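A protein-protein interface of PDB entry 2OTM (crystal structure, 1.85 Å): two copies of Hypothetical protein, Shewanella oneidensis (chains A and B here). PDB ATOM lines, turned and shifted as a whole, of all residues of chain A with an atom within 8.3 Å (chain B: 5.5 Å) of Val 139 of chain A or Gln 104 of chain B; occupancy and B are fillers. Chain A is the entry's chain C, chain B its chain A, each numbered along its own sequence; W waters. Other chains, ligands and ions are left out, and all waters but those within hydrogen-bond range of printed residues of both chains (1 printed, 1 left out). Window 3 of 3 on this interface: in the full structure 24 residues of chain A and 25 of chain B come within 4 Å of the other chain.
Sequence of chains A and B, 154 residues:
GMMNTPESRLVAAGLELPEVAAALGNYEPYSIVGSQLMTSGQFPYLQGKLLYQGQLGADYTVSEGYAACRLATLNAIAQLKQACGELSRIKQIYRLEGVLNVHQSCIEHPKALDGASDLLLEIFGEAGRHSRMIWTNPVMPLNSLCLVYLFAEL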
ATOM      1  N   GLY A  54       0.142  10.335  22.615  1.00  0.00           N
ATOM      2  CA  GLY A  54      -0.886  11.020  23.351  1.00  0.00           C
ATOM      3  C   GLY A  54      -1.505  10.123  24.395  1.00  0.00           C
ATOM      4  O   GLY A  54      -0.872   9.198  24.879  1.00  0.00           O
ATOM      5  N   GLN A  55      -2.770  10.393  24.709  1.00  0.00           N
ATOM      6  CA  GLN A  55      -3.408   9.820  25.862  1.00  0.00           C
ATOM      7  C   GLN A  55      -4.758   9.214  25.534  1.00  0.00           C
ATOM      8  O   GLN A  55      -5.558   9.827  24.811  1.00  0.00           O
ATOM      9  CB  GLN A  55      -3.603  10.941  26.871  1.00  0.00           C
ATOM     10  CG  GLN A  55      -4.141  10.494  28.193  1.00  0.00           C
ATOM     11  CD  GLN A  55      -4.257  11.636  29.145  1.00  0.00           C
ATOM     12  OE1 GLN A  55      -5.015  12.551  28.901  1.00  0.00           O
ATOM     13  NE2 GLN A  55      -3.487  11.605  30.230  1.00  0.00           N
ATOM     14  N   VAL A  99       1.764  -0.831  29.469  1.00  0.00           N
ATOM     15  CA  VAL A  99       1.619   0.497  30.081  1.00  0.00           C
ATOM     16  C   VAL A  99       0.920   1.411  29.080  1.00  0.00           C
ATOM     17  O   VAL A  99       1.308   1.445  27.912  1.00  0.00           O
ATOM     18  CB  VAL A  99       2.970   1.158  30.404  1.00  0.00           C
ATOM     19  CG1 VAL A  99       2.721   2.479  31.179  1.00  0.00           C
ATOM     20  CG2 VAL A  99       3.914   0.236  31.208  1.00  0.00           C
ATOM     21  N   LEU A 100      -0.093   2.146  29.544  1.00  0.00           N
ATOM     22  CA  LEU A 100      -0.793   3.125  28.749  1.00  0.00           C
ATOM     23  C   LEU A 100      -0.860   4.463  29.422  1.00  0.00           C
ATOM     24  O   LEU A 100      -0.853   4.535  30.644  1.00  0.00           O
ATOM     25  CB  LEU A 100      -2.238   2.659  28.492  1.00  0.00           C
ATOM     26  CG  LEU A 100      -2.346   1.456  27.528  1.00  0.00           C
ATOM     27  CD1 LEU A 100      -2.687   0.195  28.251  1.00  0.00           C
ATOM     28  CD2 LEU A 100      -3.344   1.719  26.398  1.00  0.00           C
ATOM     29  N   ASN A 101      -0.925   5.534  28.633  1.00  0.00           N
ATOM     30  CA  ASN A 101      -1.208   6.844  29.178  1.00  0.00           C
ATOM     31  C   ASN A 101      -2.698   7.047  29.001  1.00  0.00           C
ATOM     32  O   ASN A 101      -3.173   7.051  27.887  1.00  0.00           O
ATOM     33  CB  ASN A 101      -0.432   7.921  28.464  1.00  0.00           C
ATOM     34  CG  ASN A 101      -0.658   9.284  29.036  1.00  0.00           C
ATOM     35  OD1 ASN A 101      -1.378   9.470  30.034  1.00  0.00           O
ATOM     36  ND2 ASN A 101      -0.031  10.282  28.402  1.00  0.00           N
ATOM     37  N   VAL A 102      -3.411   7.233  30.113  1.00  0.00           N
ATOM     38  CA  VAL A 102      -4.871   7.172  30.133  1.00  0.00           C
ATOM     39  C   VAL A 102      -5.443   8.372  30.877  1.00  0.00           C
ATOM     40  O   VAL A 102      -5.038   8.681  31.987  1.00  0.00           O
ATOM     41  CB  VAL A 102      -5.383   5.885  30.791  1.00  0.00           C
ATOM     42  CG1 VAL A 102      -6.945   5.854  30.720  1.00  0.00           C
ATOM     43  CG2 VAL A 102      -4.761   4.654  30.105  1.00  0.00           C
ATOM     44  N   THR A 136      -1.163   2.279  34.188  1.00  0.00           N
ATOM     45  CA  THR A 136      -1.224   3.590  33.567  1.00  0.00           C
ATOM     46  C   THR A 136      -0.100   4.446  34.154  1.00  0.00           C
ATOM     47  O   THR A 136       0.156   4.397  35.336  1.00  0.00           O
ATOM     48  CB  THR A 136      -2.605   4.265  33.773  1.00  0.00           C
ATOM     49  OG1 THR A 136      -2.867   4.481  35.174  1.00  0.00           O
ATOM     50  CG2 THR A 136      -3.699   3.353  33.210  1.00  0.00           C
ATOM     51  N   ASN A 137       0.556   5.240  33.313  1.00  0.00           N
ATOM     52  CA  ASN A 137       1.572   6.158  33.763  1.00  0.00           C
ATOM     53  C   ASN A 137       1.271   7.531  33.179  1.00  0.00           C
ATOM     54  O   ASN A 137       0.752   7.616  32.080  1.00  0.00           O
ATOM     55  CB  ASN A 137       2.949   5.758  33.256  1.00  0.00           C
ATOM     56  CG  ASN A 137       3.562   4.507  33.909  1.00  0.00           C
ATOM     57  OD1 ASN A 137       4.678   4.162  33.537  1.00  0.00           O
ATOM     58  ND2 ASN A 137       2.905   3.874  34.897  1.00  0.00           N
ATOM     59  N   PRO A 138       1.592   8.600  33.907  1.00  0.00           N
ATOM     60  CA  PRO A 138       1.237   9.940  33.423  1.00  0.00           C
ATOM     61  C   PRO A 138       2.128  10.469  32.302  1.00  0.00           C
ATOM     62  O   PRO A 138       1.718  11.344  31.552  1.00  0.00           O
ATOM     63  CB  PRO A 138       1.373  10.796  34.681  1.00  0.00           C
ATOM     64  CG  PRO A 138       2.311  10.111  35.519  1.00  0.00           C
ATOM     65  CD  PRO A 138       2.169   8.649  35.258  1.00  0.00           C
ATOM     66  N   VAL A 139       3.348   9.971  32.218  1.00  0.00           N
ATOM     67  CA  VAL A 139       4.324  10.462  31.238  1.00  0.00           C
ATOM     68  C   VAL A 139       4.976   9.252  30.617  1.00  0.00           C
ATOM     69  O   VAL A 139       5.436   8.340  31.329  1.00  0.00           O
ATOM     70  CB  VAL A 139       5.409  11.330  31.941  1.00  0.00           C
ATOM     71  CG1 VAL A 139       6.523  11.832  30.934  1.00  0.00           C
ATOM     72  CG2 VAL A 139       4.737  12.512  32.695  1.00  0.00           C
ATOM     73  N   MET A 140       5.035   9.239  29.302  1.00  0.00           N
ATOM     74  CA  MET A 140       5.576   8.109  28.584  1.00  0.00           C
ATOM     75  C   MET A 140       6.815   8.489  27.765  1.00  0.00           C
ATOM     76  O   MET A 140       6.906   9.607  27.266  1.00  0.00           O
ATOM     77  CB  MET A 140       4.496   7.590  27.639  1.00  0.00           C
ATOM     78  CG  MET A 140       3.209   7.177  28.353  1.00  0.00           C
ATOM     79  SD  MET A 140       3.395   5.509  29.284  1.00  0.00           S
ATOM     80  CE  MET A 140       3.583   4.360  27.774  1.00  0.00           C
ATOM     81  N   PRO A 141       7.710   7.517  27.509  1.00  0.00           N
ATOM     82  CA  PRO A 141       8.830   7.851  26.629  1.00  0.00           C
ATOM     83  C   PRO A 141       8.258   8.189  25.247  1.00  0.00           C
ATOM     84  O   PRO A 141       7.281   7.547  24.797  1.00  0.00           O
ATOM     85  CB  PRO A 141       9.656   6.566  26.583  1.00  0.00           C
ATOM     86  CG  PRO A 141       9.083   5.686  27.666  1.00  0.00           C
ATOM     87  CD  PRO A 141       7.709   6.103  27.904  1.00  0.00           C
ATOM     88  N   LEU A 142       8.808   9.224  24.640  1.00  0.00           N
ATOM     89  CA  LEU A 142       8.419   9.688  23.290  1.00  0.00           C
ATOM     90  C   LEU A 142       6.965  10.121  23.226  1.00  0.00           C
ATOM     91  O   LEU A 142       6.418  10.285  22.138  1.00  0.00           O
ATOM     92  CB  LEU A 142       8.703   8.606  22.234  1.00  0.00           C
ATOM     93  CG  LEU A 142      10.134   8.047  22.172  1.00  0.00           C
ATOM     94  CD1 LEU A 142      10.261   6.954  21.110  1.00  0.00           C
ATOM     95  CD2 LEU A 142      11.083   9.209  21.905  1.00  0.00           C
ATOM     96  N   ASN A 143       6.340  10.350  24.379  1.00  0.00           N
ATOM     97  CA  ASN A 143       4.892  10.591  24.446  1.00  0.00           C
ATOM     98  C   ASN A 143       4.065   9.482  23.820  1.00  0.00           C
ATOM     99  O   ASN A 143       2.936   9.713  23.371  1.00  0.00           O
ATOM    100  CB  ASN A 143       4.529  11.939  23.813  1.00  0.00           C
ATOM    101  CG  ASN A 143       3.120  12.407  24.176  1.00  0.00           C
ATOM    102  OD1 ASN A 143       2.588  12.066  25.253  1.00  0.00           O
ATOM    103  ND2 ASN A 143       2.498  13.196  23.274  1.00  0.00           N
ATOM    104  N   SER A 144       4.586   8.259  23.832  1.00  0.00           N
ATOM    105  CA  SER A 144       3.868   7.141  23.260  1.00  0.00           C
ATOM    106  C   SER A 144       2.566   6.911  24.034  1.00  0.00           C
ATOM    107  O   SER A 144       2.496   7.136  25.265  1.00  0.00           O
ATOM    108  CB  SER A 144       4.712   5.877  23.292  1.00  0.00           C
ATOM    109  OG  SER A 144       4.026   4.767  22.713  1.00  0.00           O
ATOM    110  N   LEU A 147       3.240   1.178  25.762  1.00  0.00           N
ATOM    111  CA  LEU A 147       4.466   0.404  25.757  1.00  0.00           C
ATOM    112  C   LEU A 147       4.094  -1.015  26.147  1.00  0.00           C
ATOM    113  O   LEU A 147       3.371  -1.205  27.120  1.00  0.00           O
ATOM    114  CB  LEU A 147       5.399   0.927  26.830  1.00  0.00           C
ATOM    115  CG  LEU A 147       6.520   1.880  26.533  1.00  0.00           C
ATOM    116  CD1 LEU A 147       7.298   2.026  27.836  1.00  0.00           C
ATOM    117  CD2 LEU A 147       7.407   1.380  25.370  1.00  0.00           C
ATOM    118  N   VAL B 102       7.960  12.089  37.377  1.00  0.00           N
ATOM    119  CA  VAL B 102       8.268  12.959  36.267  1.00  0.00           C
ATOM    120  C   VAL B 102       7.134  13.913  35.962  1.00  0.00           C
ATOM    121  O   VAL B 102       5.969  13.511  35.851  1.00  0.00           O
ATOM    122  CB  VAL B 102       8.560  12.109  34.976  1.00  0.00           C
ATOM    123  CG1 VAL B 102       8.978  13.022  33.804  1.00  0.00           C
ATOM    124  CG2 VAL B 102       9.655  11.079  35.257  1.00  0.00           C
ATOM    125  N   HIS B 103       7.485  15.173  35.785  1.00  0.00           N
ATOM    126  CA  HIS B 103       6.546  16.229  35.450  1.00  0.00           C
ATOM    127  C   HIS B 103       6.121  16.110  33.981  1.00  0.00           C
ATOM    128  O   HIS B 103       6.904  15.688  33.135  1.00  0.00           O
ATOM    129  CB  HIS B 103       7.201  17.591  35.667  1.00  0.00           C
ATOM    130  CG  HIS B 103       6.252  18.731  35.536  1.00  0.00           C
ATOM    131  ND1 HIS B 103       6.076  19.408  34.354  1.00  0.00           N
ATOM    132  CD2 HIS B 103       5.381  19.267  36.419  1.00  0.00           C
ATOM    133  CE1 HIS B 103       5.161  20.348  34.527  1.00  0.00           C
ATOM    134  NE2 HIS B 103       4.730  20.287  35.774  1.00  0.00           N
ATOM    135  N   GLN B 104       4.883  16.492  33.687  1.00  0.00           N
ATOM    136  CA  GLN B 104       4.350  16.440  32.315  1.00  0.00           C
ATOM    137  C   GLN B 104       5.253  17.116  31.290  1.00  0.00           C
ATOM    138  O   GLN B 104       5.316  16.695  30.145  1.00  0.00           O
ATOM    139  CB  GLN B 104       2.954  17.077  32.231  1.00  0.00           C
ATOM    140  CG  GLN B 104       1.825  16.056  31.998  1.00  0.00           C
ATOM    141  N   SER B 105       5.948  18.175  31.693  1.00  0.00           N
ATOM    142  CA  SER B 105       6.812  18.934  30.767  1.00  0.00           C
ATOM    143  C   SER B 105       8.093  18.209  30.338  1.00  0.00           C
ATOM    144  O   SER B 105       8.842  18.742  29.528  1.00  0.00           O
ATOM    145  CB  SER B 105       7.231  20.258  31.405  1.00  0.00           C
ATOM    146  OG  SER B 105       8.078  20.050  32.551  1.00  0.00           O
ATOM    147  N   CYS B 106       8.360  17.023  30.879  1.00  0.00           N
ATOM    148  CA  CYS B 106       9.612  16.322  30.645  1.00  0.00           C
ATOM    149  C   CYS B 106       9.354  14.922  30.103  1.00  0.00           C
ATOM    150  O   CYS B 106       8.657  14.157  30.752  1.00  0.00           O
ATOM    151  CB  CYS B 106      10.328  16.199  32.002  1.00  0.00           C
ATOM    152  SG  CYS B 106      11.937  15.370  31.966  1.00  0.00           S
ATOM    153  N   ILE B 107       9.928  14.542  28.963  1.00  0.00           N
ATOM    154  CA  ILE B 107       9.905  13.099  28.553  1.00  0.00           C
ATOM    155  C   ILE B 107      11.328  12.546  28.396  1.00  0.00           C
ATOM    156  O   ILE B 107      11.546  11.528  27.719  1.00  0.00           O
ATOM    157  CB  ILE B 107       9.105  12.822  27.204  1.00  0.00           C
ATOM    158  CG1 ILE B 107       9.700  13.642  26.026  1.00  0.00           C
ATOM    159  CG2 ILE B 107       7.577  13.014  27.388  1.00  0.00           C
ATOM    160  CD1 ILE B 107       9.208  13.176  24.622  1.00  0.00           C
ATOM    161  N   HIS B 109      13.039  11.186  30.731  1.00  0.00           N
ATOM    162  CA  HIS B 109      13.323  10.251  31.818  1.00  0.00           C
ATOM    163  C   HIS B 109      14.093   9.036  31.391  1.00  0.00           C
ATOM    164  O   HIS B 109      14.817   8.466  32.209  1.00  0.00           O
ATOM    165  CB  HIS B 109      12.050   9.916  32.629  1.00  0.00           C
ATOM    166  CG  HIS B 109      10.931   9.350  31.821  1.00  0.00           C
ATOM    167  ND1 HIS B 109      10.226  10.093  30.893  1.00  0.00           N
ATOM    168  CD2 HIS B 109      10.375   8.119  31.816  1.00  0.00           C
ATOM    169  CE1 HIS B 109       9.308   9.331  30.335  1.00  0.00           C
ATOM    170  NE2 HIS B 109       9.392   8.124  30.862  1.00  0.00           N
ATOM    171  N   THR B 136       6.801   5.865  34.977  1.00  0.00           N
ATOM    172  CA  THR B 136       6.640   7.065  35.751  1.00  0.00           C
ATOM    173  C   THR B 136       5.442   6.887  36.670  1.00  0.00           C
ATOM    174  O   THR B 136       4.428   6.303  36.261  1.00  0.00           O
ATOM    175  CB  THR B 136       6.475   8.311  34.840  1.00  0.00           C
ATOM    176  OG1 THR B 136       5.300   8.160  34.017  1.00  0.00           O
ATOM    177  CG2 THR B 136       7.720   8.531  34.022  1.00  0.00           C
HETATM  178  O   HOH W   1       7.368   6.166  31.180  1.00  0.00           O
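Of the 16 printed residues of chain A, 6 touch a printed residue of chain B.
Hydrophobic or aromatic side chains of chain A within 4 Å of the printed part of chain B: Pro 138, Val 139 and Pro 141.
Hydrophobic or aromatic side chains of chain B within 4 Å of the printed part of chain A: Val 102, Ile 107 and His 109.
Among the printed residues, 13 pairs touch across the chains.
Water W1 lies within hydrogen-bond range of a ring nitrogen (NE2) of His 109 of chain B (2.8 Å) and the backbone carbonyl oxygen of Val 139 of chain A (2.9 Å).
Among the printed residues, pairs that only touch across the chains: Val 139 of chain A with Cys 106 of chain B (3.2 Å), Pro 138 of chain A with Thr 136 of chain B (3.4 Å), Met 140 of chain A with Ile 107 of chain B (3.5 Å), Val 139 of chain A with Val 102 of chain B (3.5 Å), Met 140 of chain A with His 109 of chain B (3.7 Å), Pro 141 of chain A with His 109 of chain B (3.7 Å), Val 139 of chain A with His 109 of chain B (3.8 Å), Leu 142 of chain A with Ile 107 of chain B (3.8 Å), Val 139 of chain A with His 103 of chain B (3.9 Å), Val 139 of chain A with Ile 107 of chain B (3.9 Å) and Val 139 of chain A with Gln 104 of chain B (3.97 Å).
ND1 of His 103 of chain B is in hydrogen-bond range of OG of Ser 105 of chain B, at 2.8 Å.
O of Leu 100 of chain A sits at hydrogen-bond distance from N of Asn 137 of chain A, 3.1 Å away.
The side-chain amide oxygen of Asn 101 of chain A sits close to the backbone carbonyl oxygen of Asn 137 of chain A (3.5 Å).
2 positions are printed for both chains.
Of the 13 pairs that touch across the chains among the printed residues, none has its exchanged pair printed and touching as well.
Of chain B, only Val 102 (3.5 Å), His 103 (3.9 Å), Gln 104 (3.97 Å), Cys 106 (3.2 Å), Ile 107 (3.9 Å), His 109 (3.8 Å) and Thr 136 (2.7 Å) come within 4 Å of Val 139 of chain A.
Of the printed residues of chain A, Gln 104 of chain B touches Val 139.
Printed residues of chain A within 4 Å of His 103 of chain B: Val 139 (3.9 Å).
Printed residues of chain A within 4 Å of His 109 of chain B: Val 139, Met 140 and Pro 141.
Printed residues of chain B within 4 Å of Leu 142 of chain A: Ile 107 (3.8 Å).
Printed residues of chain B within 4 Å of Pro 138 of chain A: Thr 136 (3.4 Å).
Leu 100 of chain A touches none of the printed residues of chain B.
The nearest printed residue of chain A that does not touch Val 102 of chain B is Pro 138 of chain A (5.0 Å).
N of Thr 136 of chain B is in hydrogen-bond range of OD1 of Asn 137 of chain A, 3.1 Å away.
The side-chain hydroxyl (OG1) of Thr 136 of chain B is in hydrogen-bond range of the backbone carbonyl oxygen (O) of Val 139 of chain A, at 2.7 Å.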
